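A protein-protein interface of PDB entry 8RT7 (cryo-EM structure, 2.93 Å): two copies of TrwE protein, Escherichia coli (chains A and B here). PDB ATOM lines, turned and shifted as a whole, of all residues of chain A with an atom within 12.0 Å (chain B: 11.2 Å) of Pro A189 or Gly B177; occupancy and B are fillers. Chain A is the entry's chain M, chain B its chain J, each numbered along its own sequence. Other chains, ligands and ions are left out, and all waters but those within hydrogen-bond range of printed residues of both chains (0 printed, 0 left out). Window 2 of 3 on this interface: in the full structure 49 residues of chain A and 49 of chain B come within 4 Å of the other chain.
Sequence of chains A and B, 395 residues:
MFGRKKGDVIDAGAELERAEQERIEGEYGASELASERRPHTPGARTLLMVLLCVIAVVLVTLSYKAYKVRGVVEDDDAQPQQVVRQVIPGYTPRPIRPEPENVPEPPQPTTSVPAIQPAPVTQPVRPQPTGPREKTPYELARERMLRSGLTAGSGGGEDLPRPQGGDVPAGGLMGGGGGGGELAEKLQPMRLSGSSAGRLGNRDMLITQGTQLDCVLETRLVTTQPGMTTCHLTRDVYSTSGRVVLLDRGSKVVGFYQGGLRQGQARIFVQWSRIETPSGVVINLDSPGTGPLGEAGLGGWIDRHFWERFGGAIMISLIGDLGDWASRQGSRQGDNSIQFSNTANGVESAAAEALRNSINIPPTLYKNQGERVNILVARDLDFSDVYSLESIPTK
The backbone NH (N) of Gly B179 is in hydrogen-bond range of the backbone carbonyl oxygen (O) of Pro A189, 2.9 Å away.
Positions printed for both chains: 181, 182, 183, 184, 185 and 188.
Of the 8 pairs that touch across the chains among the printed residues, none has its exchanged pair printed and touching as well.
The backbone carbonyl oxygen of Ala B184 lies within hydrogen-bond range of the side-chain amide nitrogen of Gln B188 (2.8 Å).
Printed residues of chain B within 4 Å of Pro A189: Gly B177, Gly B178 and Gly B179.
Gly B177 touches just these residues of chain A: Pro A189 and Arg A191.
Of chain B, only Gly B179, Gly B180, Leu B183 and Ala B184 come within 4 Å of Met A190.
Of the printed residues of chain A, Gly B180 touches Met A190 (3.9 Å).
Printed residues of chain A within 4 Å of Ala B184: Met A190.
Printed residues of chain A within 4 Å of Leu B183: Met A190 (3.7 Å).
The nearest residue of chain B that does not touch Pro A189 is Gly B180 (4.4 Å).
The nearest printed residue of chain A that does not touch Leu B183 is Leu A192 (6.4 Å).
Among the printed residues, pairs that only touch across the chains: Pro A189 with Gly B177 (3.5 Å), Met A190 with Gly B179 (3.6 Å), Arg A191 with Gly B177 (3.7 Å), Met A190 with Leu B183 (3.7 Å), Met A190 with Ala B184 (3.8 Å), Pro A189 with Gly B178 (3.8 Å) and Met A190 with Gly B180 (3.9 Å).
Of the 14 printed residues of chain A, 3 touch a printed residue of chain B.
Hydrophobic or aromatic side chains of chain A that line the printed part of chain B: Pro A189 and Met A190.
Among the printed residues, 8 pairs touch across the chains.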
ATOM      1  N   GLY A 181     -15.123   2.568   2.298  1.00  0.00           N
ATOM      2  CA  GLY A 181     -15.689   2.197   3.587  1.00  0.00           C
ATOM      3  C   GLY A 181     -17.099   1.649   3.498  1.00  0.00           C
ATOM      4  O   GLY A 181     -17.414   0.627   4.105  1.00  0.00           O
ATOM      5  N   GLU A 182     -17.969   2.324   2.747  1.00  0.00           N
ATOM      6  CA  GLU A 182     -19.350   1.865   2.631  1.00  0.00           C
ATOM      7  C   GLU A 182     -19.443   0.549   1.881  1.00  0.00           C
ATOM      8  O   GLU A 182     -20.065  -0.408   2.356  1.00  0.00           O
ATOM      9  CB  GLU A 182     -20.196   2.920   1.932  1.00  0.00           C
ATOM     10  CG  GLU A 182     -21.623   2.940   2.378  1.00  0.00           C
ATOM     11  CD  GLU A 182     -22.503   3.706   1.429  1.00  0.00           C
ATOM     12  OE1 GLU A 182     -22.003   4.653   0.795  1.00  0.00           O
ATOM     13  OE2 GLU A 182     -23.698   3.368   1.322  1.00  0.00           O
ATOM     14  N   LEU A 183     -18.827   0.477   0.706  1.00  0.00           N
ATOM     15  CA  LEU A 183     -18.968  -0.711  -0.121  1.00  0.00           C
ATOM     16  C   LEU A 183     -18.283  -1.911   0.514  1.00  0.00           C
ATOM     17  O   LEU A 183     -18.782  -3.033   0.417  1.00  0.00           O
ATOM     18  CB  LEU A 183     -18.424  -0.440  -1.518  1.00  0.00           C
ATOM     19  CG  LEU A 183     -18.402  -1.594  -2.510  1.00  0.00           C
ATOM     20  CD1 LEU A 183     -19.760  -2.199  -2.674  1.00  0.00           C
ATOM     21  CD2 LEU A 183     -17.893  -1.103  -3.818  1.00  0.00           C
ATOM     22  N   ALA A 184     -17.144  -1.701   1.169  1.00  0.00           N
ATOM     23  CA  ALA A 184     -16.450  -2.814   1.801  1.00  0.00           C
ATOM     24  C   ALA A 184     -17.129  -3.269   3.077  1.00  0.00           C
ATOM     25  O   ALA A 184     -16.898  -4.399   3.511  1.00  0.00           O
ATOM     26  CB  ALA A 184     -15.005  -2.443   2.108  1.00  0.00           C
ATOM     27  N   GLU A 185     -17.933  -2.414   3.700  1.00  0.00           N
ATOM     28  CA  GLU A 185     -18.725  -2.839   4.842  1.00  0.00           C
ATOM     29  C   GLU A 185     -19.963  -3.593   4.398  1.00  0.00           C
ATOM     30  O   GLU A 185     -20.440  -4.484   5.104  1.00  0.00           O
ATOM     31  CB  GLU A 185     -19.127  -1.638   5.686  1.00  0.00           C
ATOM     32  CG  GLU A 185     -18.227  -1.373   6.866  1.00  0.00           C
ATOM     33  CD  GLU A 185     -18.447   0.006   7.452  1.00  0.00           C
ATOM     34  OE1 GLU A 185     -17.541   0.510   8.150  1.00  0.00           O
ATOM     35  OE2 GLU A 185     -19.528   0.584   7.216  1.00  0.00           O
ATOM     36  N   LYS A 186     -20.514  -3.232   3.243  1.00  0.00           N
ATOM     37  CA  LYS A 186     -21.629  -3.995   2.707  1.00  0.00           C
ATOM     38  C   LYS A 186     -21.206  -5.338   2.145  1.00  0.00           C
ATOM     39  O   LYS A 186     -22.072  -6.176   1.891  1.00  0.00           O
ATOM     40  CB  LYS A 186     -22.343  -3.191   1.635  1.00  0.00           C
ATOM     41  CG  LYS A 186     -23.207  -2.110   2.189  1.00  0.00           C
ATOM     42  CD  LYS A 186     -23.976  -1.434   1.105  1.00  0.00           C
ATOM     43  CE  LYS A 186     -25.311  -0.966   1.618  1.00  0.00           C
ATOM     44  NZ  LYS A 186     -26.007  -2.054   2.339  1.00  0.00           N
ATOM     45  N   LEU A 187     -19.914  -5.565   1.950  1.00  0.00           N
ATOM     46  CA  LEU A 187     -19.412  -6.829   1.439  1.00  0.00           C
ATOM     47  C   LEU A 187     -18.794  -7.696   2.523  1.00  0.00           C
ATOM     48  O   LEU A 187     -18.120  -8.673   2.202  1.00  0.00           O
ATOM     49  CB  LEU A 187     -18.393  -6.593   0.329  1.00  0.00           C
ATOM     50  CG  LEU A 187     -18.941  -6.151  -1.021  1.00  0.00           C
ATOM     51  CD1 LEU A 187     -17.834  -6.077  -2.022  1.00  0.00           C
ATOM     52  CD2 LEU A 187     -20.015  -7.086  -1.476  1.00  0.00           C
ATOM     53  N   GLN A 188     -18.989  -7.354   3.787  1.00  0.00           N
ATOM     54  CA  GLN A 188     -18.590  -8.244   4.864  1.00  0.00           C
ATOM     55  C   GLN A 188     -19.409  -9.524   4.771  1.00  0.00           C
ATOM     56  O   GLN A 188     -20.641  -9.455   4.703  1.00  0.00           O
ATOM     57  CB  GLN A 188     -18.807  -7.586   6.223  1.00  0.00           C
ATOM     58  CG  GLN A 188     -17.771  -6.559   6.611  1.00  0.00           C
ATOM     59  CD  GLN A 188     -16.375  -6.921   6.151  1.00  0.00           C
ATOM     60  OE1 GLN A 188     -15.830  -7.954   6.532  1.00  0.00           O
ATOM     61  NE2 GLN A 188     -15.789  -6.069   5.323  1.00  0.00           N
ATOM     62  N   PRO A 189     -18.780 -10.692   4.757  1.00  0.00           N
ATOM     63  CA  PRO A 189     -19.535 -11.930   4.576  1.00  0.00           C
ATOM     64  C   PRO A 189     -20.380 -12.259   5.791  1.00  0.00           C
ATOM     65  O   PRO A 189     -20.170 -11.753   6.893  1.00  0.00           O
ATOM     66  CB  PRO A 189     -18.446 -12.977   4.364  1.00  0.00           C
ATOM     67  CG  PRO A 189     -17.280 -12.430   5.045  1.00  0.00           C
ATOM     68  CD  PRO A 189     -17.342 -10.950   4.907  1.00  0.00           C
ATOM     69  N   MET A 190     -21.371 -13.103   5.564  1.00  0.00           N
ATOM     70  CA  MET A 190     -22.183 -13.678   6.626  1.00  0.00           C
ATOM     71  C   MET A 190     -21.964 -15.179   6.554  1.00  0.00           C
ATOM     72  O   MET A 190     -22.517 -15.851   5.681  1.00  0.00           O
ATOM     73  CB  MET A 190     -23.652 -13.320   6.462  1.00  0.00           C
ATOM     74  CG  MET A 190     -24.529 -13.842   7.563  1.00  0.00           C
ATOM     75  SD  MET A 190     -26.238 -13.382   7.349  1.00  0.00           S
ATOM     76  CE  MET A 190     -26.662 -14.431   5.988  1.00  0.00           C
ATOM     77  N   ARG A 191     -21.140 -15.698   7.453  1.00  0.00           N
ATOM     78  CA  ARG A 191     -20.785 -17.109   7.471  1.00  0.00           C
ATOM     79  C   ARG A 191     -21.638 -17.800   8.521  1.00  0.00           C
ATOM     80  O   ARG A 191     -21.423 -17.618   9.722  1.00  0.00           O
ATOM     81  CB  ARG A 191     -19.303 -17.294   7.773  1.00  0.00           C
ATOM     82  CG  ARG A 191     -18.382 -16.631   6.790  1.00  0.00           C
ATOM     83  CD  ARG A 191     -18.537 -17.214   5.409  1.00  0.00           C
ATOM     84  NE  ARG A 191     -17.792 -16.451   4.413  1.00  0.00           N
ATOM     85  CZ  ARG A 191     -16.468 -16.372   4.360  1.00  0.00           C
ATOM     86  NH1 ARG A 191     -15.719 -17.019   5.237  1.00  0.00           N
ATOM     87  NH2 ARG A 191     -15.887 -15.652   3.416  1.00  0.00           N
ATOM     88  N   LEU A 192     -22.597 -18.596   8.071  1.00  0.00           N
ATOM     89  CA  LEU A 192     -23.476 -19.342   8.955  1.00  0.00           C
ATOM     90  C   LEU A 192     -22.972 -20.773   9.028  1.00  0.00           C
ATOM     91  O   LEU A 192     -22.847 -21.442   7.999  1.00  0.00           O
ATOM     92  CB  LEU A 192     -24.918 -19.289   8.459  1.00  0.00           C
ATOM     93  CG  LEU A 192     -25.510 -17.892   8.344  1.00  0.00           C
ATOM     94  CD1 LEU A 192     -26.883 -17.957   7.769  1.00  0.00           C
ATOM     95  CD2 LEU A 192     -25.546 -17.238   9.696  1.00  0.00           C
ATOM     96  N   SER A 193     -22.679 -21.231  10.236  1.00  0.00           N
ATOM     97  CA  SER A 193     -22.037 -22.519  10.416  1.00  0.00           C
ATOM     98  C   SER A 193     -23.032 -23.651  10.218  1.00  0.00           C
ATOM     99  O   SER A 193     -24.214 -23.532  10.539  1.00  0.00           O
ATOM    100  CB  SER A 193     -21.414 -22.600  11.802  1.00  0.00           C
ATOM    101  OG  SER A 193     -22.408 -22.496  12.798  1.00  0.00           O
ATOM    102  N   GLY A 194     -22.542 -24.761   9.691  1.00  0.00           N
ATOM    103  CA  GLY A 194     -23.406 -25.866   9.352  1.00  0.00           C
ATOM    104  C   GLY A 194     -23.924 -26.600  10.565  1.00  0.00           C
ATOM    105  O   GLY A 194     -23.490 -26.395  11.694  1.00  0.00           O
ATOM    106  N   GLY B 177     -16.221 -14.037   8.600  1.00  0.00           N
ATOM    107  CA  GLY B 177     -16.898 -12.755   8.622  1.00  0.00           C
ATOM    108  C   GLY B 177     -18.116 -12.737   9.522  1.00  0.00           C
ATOM    109  O   GLY B 177     -18.861 -13.712   9.592  1.00  0.00           O
ATOM    110  N   GLY B 178     -18.308 -11.622  10.224  1.00  0.00           N
ATOM    111  CA  GLY B 178     -19.440 -11.451  11.112  1.00  0.00           C
ATOM    112  C   GLY B 178     -20.565 -10.593  10.584  1.00  0.00           C
ATOM    113  O   GLY B 178     -21.493 -10.285  11.344  1.00  0.00           O
ATOM    114  N   GLY B 179     -20.535 -10.202   9.312  1.00  0.00           N
ATOM    115  CA  GLY B 179     -21.530  -9.305   8.760  1.00  0.00           C
ATOM    116  C   GLY B 179     -22.912  -9.904   8.615  1.00  0.00           C
ATOM    117  O   GLY B 179     -23.234 -10.907   9.257  1.00  0.00           O
ATOM    118  N   GLY B 180     -23.738  -9.305   7.765  1.00  0.00           N
ATOM    119  CA  GLY B 180     -25.140  -9.660   7.724  1.00  0.00           C
ATOM    120  C   GLY B 180     -25.807  -9.308   9.034  1.00  0.00           C
ATOM    121  O   GLY B 180     -26.580 -10.098   9.574  1.00  0.00           O
ATOM    122  N   GLY B 181     -25.535  -8.101   9.532  1.00  0.00           N
ATOM    123  CA  GLY B 181     -25.780  -7.800  10.932  1.00  0.00           C
ATOM    124  C   GLY B 181     -27.225  -7.955  11.358  1.00  0.00           C
ATOM    125  O   GLY B 181     -27.499  -8.377  12.481  1.00  0.00           O
ATOM    126  N   GLU B 182     -28.168  -7.597  10.490  1.00  0.00           N
ATOM    127  CA  GLU B 182     -29.569  -7.686  10.886  1.00  0.00           C
ATOM    128  C   GLU B 182     -30.140  -9.066  10.600  1.00  0.00           C
ATOM    129  O   GLU B 182     -30.805  -9.664  11.451  1.00  0.00           O
ATOM    130  CB  GLU B 182     -30.394  -6.616  10.183  1.00  0.00           C
ATOM    131  CG  GLU B 182     -31.872  -6.911  10.204  1.00  0.00           C
ATOM    132  CD  GLU B 182     -32.682  -5.915   9.415  1.00  0.00           C
ATOM    133  OE1 GLU B 182     -32.154  -5.352   8.437  1.00  0.00           O
ATOM    134  OE2 GLU B 182     -33.855  -5.701   9.774  1.00  0.00           O
ATOM    135  N   LEU B 183     -29.873  -9.593   9.409  1.00  0.00           N
ATOM    136  CA  LEU B 183     -30.339 -10.931   9.079  1.00  0.00           C
ATOM    137  C   LEU B 183     -29.710 -11.978   9.989  1.00  0.00           C
ATOM    138  O   LEU B 183     -30.382 -12.926  10.400  1.00  0.00           O
ATOM    139  CB  LEU B 183     -30.045 -11.240   7.616  1.00  0.00           C
ATOM    140  CG  LEU B 183     -30.406 -12.646   7.159  1.00  0.00           C
ATOM    141  CD1 LEU B 183     -31.860 -12.935   7.377  1.00  0.00           C
ATOM    142  CD2 LEU B 183     -30.029 -12.832   5.728  1.00  0.00           C
ATOM    143  N   ALA B 184     -28.425 -11.841  10.305  1.00  0.00           N
ATOM    144  CA  ALA B 184     -27.778 -12.821  11.165  1.00  0.00           C
ATOM    145  C   ALA B 184     -28.178 -12.677  12.619  1.00  0.00           C
ATOM    146  O   ALA B 184     -28.050 -13.639  13.378  1.00  0.00           O
ATOM    147  CB  ALA B 184     -26.261 -12.720  11.056  1.00  0.00           C
ATOM    148  N   GLU B 185     -28.623 -11.494  13.032  1.00  0.00           N
ATOM    149  CA  GLU B 185     -29.161 -11.341  14.373  1.00  0.00           C
ATOM    150  C   GLU B 185     -30.565 -11.910  14.463  1.00  0.00           C
ATOM    151  O   GLU B 185     -30.987 -12.351  15.533  1.00  0.00           O
ATOM    152  CB  GLU B 185     -29.146  -9.873  14.775  1.00  0.00           C
ATOM    153  CG  GLU B 185     -29.449  -9.622  16.232  1.00  0.00           C
ATOM    154  CD  GLU B 185     -30.112  -8.284  16.469  1.00  0.00           C
ATOM    155  OE1 GLU B 185     -30.587  -8.052  17.600  1.00  0.00           O
ATOM    156  OE2 GLU B 185     -30.152  -7.462  15.529  1.00  0.00           O
ATOM    157  N   GLN B 188     -30.387 -15.986  15.021  1.00  0.00           N
ATOM    158  CA  GLN B 188     -29.810 -16.590  16.211  1.00  0.00           C
ATOM    159  C   GLN B 188     -30.755 -17.655  16.744  1.00  0.00           C
ATOM    160  O   GLN B 188     -31.935 -17.373  16.960  1.00  0.00           O
ATOM    161  CB  GLN B 188     -29.543 -15.549  17.286  1.00  0.00           C
ATOM    162  CG  GLN B 188     -28.313 -14.703  17.054  1.00  0.00           C
ATOM    163  CD  GLN B 188     -27.165 -15.476  16.427  1.00  0.00           C
ATOM    164  OE1 GLN B 188     -26.789 -16.550  16.895  1.00  0.00           O
ATOM    165  NE2 GLN B 188     -26.602 -14.926  15.360  1.00  0.00           N
